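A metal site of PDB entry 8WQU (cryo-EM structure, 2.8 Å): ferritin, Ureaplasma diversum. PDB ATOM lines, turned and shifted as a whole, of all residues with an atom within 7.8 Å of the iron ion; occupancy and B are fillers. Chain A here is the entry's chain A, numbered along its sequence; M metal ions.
O of His 65 sits at hydrogen-bond distance from ND2 of Asn 27 (3.5 Å).
The backbone carbonyl oxygen (O) of His 65 sits at hydrogen-bond distance from the side-chain hydroxyl (OH) of Tyr 135.
The iron ion is bound by a ring nitrogen (NE2) of His 65 (2.1 Å), the side-chain carboxylate of Asp 138 (2.4 Å) and the side-chain carboxylate of Asp 142 (2.4 Å).
The iron ion has three donor atoms within binding distance.
The nearest printed residue that does not touch the iron ion is Asp 60 (4.3 Å).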
ATOM      1  N   ASN A  27       3.341 -23.928   8.375  1.00  0.00           N
ATOM      2  CA  ASN A  27       2.888 -24.090   9.751  1.00  0.00           C
ATOM      3  C   ASN A  27       3.743 -23.281  10.723  1.00  0.00           C
ATOM      4  O   ASN A  27       3.210 -22.612  11.615  1.00  0.00           O
ATOM      5  CB  ASN A  27       2.905 -25.571  10.137  1.00  0.00           C
ATOM      6  CG  ASN A  27       1.578 -26.237   9.894  1.00  0.00           C
ATOM      7  OD1 ASN A  27       0.540 -25.599   9.970  1.00  0.00           O
ATOM      8  ND2 ASN A  27       1.614 -27.522   9.597  1.00  0.00           N
ATOM      9  N   HIS A  56      -3.775 -20.206  21.950  1.00  0.00           N
ATOM     10  CA  HIS A  56      -3.986 -21.642  21.827  1.00  0.00           C
ATOM     11  C   HIS A  56      -3.822 -22.104  20.388  1.00  0.00           C
ATOM     12  O   HIS A  56      -3.210 -23.151  20.117  1.00  0.00           O
ATOM     13  CB  HIS A  56      -5.379 -22.001  22.347  1.00  0.00           C
ATOM     14  CG  HIS A  56      -5.684 -23.466  22.304  1.00  0.00           C
ATOM     15  ND1 HIS A  56      -4.739 -24.429  22.594  1.00  0.00           N
ATOM     16  CD2 HIS A  56      -6.826 -24.127  22.014  1.00  0.00           C
ATOM     17  CE1 HIS A  56      -5.292 -25.625  22.480  1.00  0.00           C
ATOM     18  NE2 HIS A  56      -6.553 -25.477  22.131  1.00  0.00           N
ATOM     19  N   LEU A  57      -4.350 -21.319  19.438  1.00  0.00           N
ATOM     20  CA  LEU A  57      -4.131 -21.634  18.027  1.00  0.00           C
ATOM     21  C   LEU A  57      -2.631 -21.686  17.696  1.00  0.00           C
ATOM     22  O   LEU A  57      -2.169 -22.595  17.005  1.00  0.00           O
ATOM     23  CB  LEU A  57      -4.825 -20.607  17.136  1.00  0.00           C
ATOM     24  CG  LEU A  57      -6.333 -20.491  17.130  1.00  0.00           C
ATOM     25  CD1 LEU A  57      -6.742 -19.511  16.060  1.00  0.00           C
ATOM     26  CD2 LEU A  57      -6.972 -21.835  16.905  1.00  0.00           C
ATOM     27  N   GLU A  59      -0.050 -22.240  19.634  1.00  0.00           N
ATOM     28  CA  GLU A  59       0.621 -23.390  20.210  1.00  0.00           C
ATOM     29  C   GLU A  59       0.302 -24.666  19.452  1.00  0.00           C
ATOM     30  O   GLU A  59       1.192 -25.494  19.211  1.00  0.00           O
ATOM     31  CB  GLU A  59       0.247 -23.525  21.686  1.00  0.00           C
ATOM     32  CG  GLU A  59       0.896 -22.487  22.563  1.00  0.00           C
ATOM     33  CD  GLU A  59       0.453 -22.571  23.999  1.00  0.00           C
ATOM     34  OE1 GLU A  59       1.003 -21.844  24.842  1.00  0.00           O
ATOM     35  OE2 GLU A  59      -0.460 -23.377  24.290  1.00  0.00           O
ATOM     36  N   ASP A  60      -0.954 -24.858  19.048  1.00  0.00           N
ATOM     37  CA  ASP A  60      -1.274 -26.009  18.197  1.00  0.00           C
ATOM     38  C   ASP A  60      -0.438 -26.005  16.938  1.00  0.00           C
ATOM     39  O   ASP A  60       0.140 -27.035  16.556  1.00  0.00           O
ATOM     40  CB  ASP A  60      -2.760 -26.049  17.858  1.00  0.00           C
ATOM     41  CG  ASP A  60      -3.627 -26.470  19.018  1.00  0.00           C
ATOM     42  OD1 ASP A  60      -3.139 -27.212  19.900  1.00  0.00           O
ATOM     43  OD2 ASP A  60      -4.811 -26.078  19.050  1.00  0.00           O
ATOM     44  N   LYS A  61      -0.360 -24.860  16.248  1.00  0.00           N
ATOM     45  CA  LYS A  61       0.357 -24.835  14.967  1.00  0.00           C
ATOM     46  C   LYS A  61       1.840 -25.110  15.160  1.00  0.00           C
ATOM     47  O   LYS A  61       2.450 -25.822  14.356  1.00  0.00           O
ATOM     48  CB  LYS A  61       0.156 -23.496  14.279  1.00  0.00           C
ATOM     49  CG  LYS A  61      -1.278 -23.212  13.921  1.00  0.00           C
ATOM     50  CD  LYS A  61      -1.752 -24.086  12.790  1.00  0.00           C
ATOM     51  CE  LYS A  61      -3.238 -23.892  12.548  1.00  0.00           C
ATOM     52  NZ  LYS A  61      -3.720 -24.732  11.438  1.00  0.00           N
ATOM     53  N   VAL A  64       2.144 -30.017  17.370  1.00  0.00           N
ATOM     54  CA  VAL A  64       1.946 -31.325  16.749  1.00  0.00           C
ATOM     55  C   VAL A  64       1.871 -31.238  15.231  1.00  0.00           C
ATOM     56  O   VAL A  64       2.240 -32.182  14.531  1.00  0.00           O
ATOM     57  CB  VAL A  64       0.693 -32.007  17.328  1.00  0.00           C
ATOM     58  CG1 VAL A  64       0.845 -32.212  18.816  1.00  0.00           C
ATOM     59  CG2 VAL A  64      -0.545 -31.192  17.030  1.00  0.00           C
ATOM     60  N   HIS A  65       1.447 -30.087  14.686  1.00  0.00           N
ATOM     61  CA  HIS A  65       1.279 -29.970  13.241  1.00  0.00           C
ATOM     62  C   HIS A  65       2.592 -30.107  12.485  1.00  0.00           C
ATOM     63  O   HIS A  65       2.571 -30.421  11.293  1.00  0.00           O
ATOM     64  CB  HIS A  65       0.619 -28.642  12.880  1.00  0.00           C
ATOM     65  CG  HIS A  65      -0.852 -28.619  13.094  1.00  0.00           C
ATOM     66  ND1 HIS A  65      -1.741 -28.425  12.073  1.00  0.00           N
ATOM     67  CD2 HIS A  65      -1.593 -28.762  14.223  1.00  0.00           C
ATOM     68  CE1 HIS A  65      -2.975 -28.452  12.552  1.00  0.00           C
ATOM     69  NE2 HIS A  65      -2.910 -28.660  13.849  1.00  0.00           N
ATOM     70  N   GLU A 106      -6.872 -19.716   7.978  1.00  0.00           N
ATOM     71  CA  GLU A 106      -7.329 -21.102   8.095  1.00  0.00           C
ATOM     72  C   GLU A 106      -7.943 -21.606   6.788  1.00  0.00           C
ATOM     73  O   GLU A 106      -7.710 -22.758   6.369  1.00  0.00           O
ATOM     74  CB  GLU A 106      -8.327 -21.214   9.247  1.00  0.00           C
ATOM     75  CG  GLU A 106      -7.714 -20.960  10.607  1.00  0.00           C
ATOM     76  CD  GLU A 106      -6.699 -22.007  10.980  1.00  0.00           C
ATOM     77  OE1 GLU A 106      -6.928 -23.192  10.683  1.00  0.00           O
ATOM     78  OE2 GLU A 106      -5.660 -21.647  11.561  1.00  0.00           O
ATOM     79  N   TRP A 134      -5.484 -37.070   8.441  1.00  0.00           N
ATOM     80  CA  TRP A 134      -5.522 -36.336   9.704  1.00  0.00           C
ATOM     81  C   TRP A 134      -5.629 -34.835   9.471  1.00  0.00           C
ATOM     82  O   TRP A 134      -6.421 -34.142  10.106  1.00  0.00           O
ATOM     83  CB  TRP A 134      -4.293 -36.659  10.545  1.00  0.00           C
ATOM     84  CG  TRP A 134      -4.387 -36.199  11.965  1.00  0.00           C
ATOM     85  CD1 TRP A 134      -4.919 -36.890  12.997  1.00  0.00           C
ATOM     86  CD2 TRP A 134      -3.937 -34.949  12.485  1.00  0.00           C
ATOM     87  NE1 TRP A 134      -4.835 -36.150  14.151  1.00  0.00           N
ATOM     88  CE2 TRP A 134      -4.231 -34.950  13.862  1.00  0.00           C
ATOM     89  CE3 TRP A 134      -3.310 -33.827  11.946  1.00  0.00           C
ATOM     90  CZ2 TRP A 134      -3.932 -33.880  14.693  1.00  0.00           C
ATOM     91  CZ3 TRP A 134      -3.016 -32.763  12.770  1.00  0.00           C
ATOM     92  CH2 TRP A 134      -3.327 -32.795  14.126  1.00  0.00           C
ATOM     93  N   TYR A 135      -4.814 -34.316   8.550  1.00  0.00           N
ATOM     94  CA  TYR A 135      -4.840 -32.892   8.251  1.00  0.00           C
ATOM     95  C   TYR A 135      -6.120 -32.501   7.523  1.00  0.00           C
ATOM     96  O   TYR A 135      -6.673 -31.425   7.771  1.00  0.00           O
ATOM     97  CB  TYR A 135      -3.604 -32.529   7.432  1.00  0.00           C
ATOM     98  CG  TYR A 135      -2.326 -32.688   8.217  1.00  0.00           C
ATOM     99  CD1 TYR A 135      -1.726 -33.927   8.362  1.00  0.00           C
ATOM    100  CD2 TYR A 135      -1.722 -31.609   8.834  1.00  0.00           C
ATOM    101  CE1 TYR A 135      -0.573 -34.082   9.082  1.00  0.00           C
ATOM    102  CE2 TYR A 135      -0.567 -31.749   9.555  1.00  0.00           C
ATOM    103  CZ  TYR A 135       0.003 -32.980   9.671  1.00  0.00           C
ATOM    104  OH  TYR A 135       1.156 -33.135  10.390  1.00  0.00           O
ATOM    105  N   ASP A 138      -8.559 -32.127  10.443  1.00  0.00           N
ATOM    106  CA  ASP A 138      -8.295 -31.058  11.406  1.00  0.00           C
ATOM    107  C   ASP A 138      -8.489 -29.690  10.779  1.00  0.00           C
ATOM    108  O   ASP A 138      -8.790 -28.730  11.490  1.00  0.00           O
ATOM    109  CB  ASP A 138      -6.889 -31.202  11.979  1.00  0.00           C
ATOM    110  CG  ASP A 138      -6.740 -30.496  13.296  1.00  0.00           C
ATOM    111  OD1 ASP A 138      -7.255 -31.008  14.310  1.00  0.00           O
ATOM    112  OD2 ASP A 138      -6.101 -29.429  13.339  1.00  0.00           O
ATOM    113  N   GLY A 139      -8.346 -29.584   9.449  1.00  0.00           N
ATOM    114  CA  GLY A 139      -8.630 -28.316   8.808  1.00  0.00           C
ATOM    115  C   GLY A 139     -10.052 -27.851   9.054  1.00  0.00           C
ATOM    116  O   GLY A 139     -10.277 -26.724   9.506  1.00  0.00           O
ATOM    117  N   LYS A 141     -12.123 -28.929  11.326  1.00  0.00           N
ATOM    118  CA  LYS A 141     -12.352 -28.715  12.756  1.00  0.00           C
ATOM    119  C   LYS A 141     -11.913 -27.319  13.201  1.00  0.00           C
ATOM    120  O   LYS A 141     -12.677 -26.579  13.836  1.00  0.00           O
ATOM    121  CB  LYS A 141     -11.619 -29.783  13.564  1.00  0.00           C
ATOM    122  CG  LYS A 141     -11.619 -29.524  15.046  1.00  0.00           C
ATOM    123  CD  LYS A 141     -11.196 -30.748  15.804  1.00  0.00           C
ATOM    124  CE  LYS A 141     -11.453 -30.593  17.291  1.00  0.00           C
ATOM    125  NZ  LYS A 141     -11.115 -31.844  18.030  1.00  0.00           N
ATOM    126  N   ASP A 142     -10.677 -26.932  12.861  1.00  0.00           N
ATOM    127  CA  ASP A 142     -10.160 -25.642  13.313  1.00  0.00           C
ATOM    128  C   ASP A 142     -10.910 -24.487  12.669  1.00  0.00           C
ATOM    129  O   ASP A 142     -11.171 -23.476  13.323  1.00  0.00           O
ATOM    130  CB  ASP A 142      -8.667 -25.546  13.024  1.00  0.00           C
ATOM    131  CG  ASP A 142      -7.841 -26.423  13.931  1.00  0.00           C
ATOM    132  OD1 ASP A 142      -8.335 -26.787  15.013  1.00  0.00           O
ATOM    133  OD2 ASP A 142      -6.696 -26.754  13.571  1.00  0.00           O
ATOM    134  N   GLU A 145     -14.204 -24.045  14.623  1.00  0.00           N
ATOM    135  CA  GLU A 145     -14.105 -23.402  15.926  1.00  0.00           C
ATOM    136  C   GLU A 145     -13.576 -21.973  15.839  1.00  0.00           C
ATOM    137  O   GLU A 145     -13.697 -21.234  16.824  1.00  0.00           O
ATOM    138  CB  GLU A 145     -13.240 -24.232  16.868  1.00  0.00           C
ATOM    139  CG  GLU A 145     -11.781 -24.310  16.515  1.00  0.00           C
ATOM    140  CD  GLU A 145     -11.000 -25.132  17.511  1.00  0.00           C
ATOM    141  OE1 GLU A 145     -11.634 -25.721  18.407  1.00  0.00           O
ATOM    142  OE2 GLU A 145      -9.760 -25.173  17.404  1.00  0.00           O
HETATM  143 FE    FE M   1      -4.728 -27.861  14.469  1.00  0.00          FE
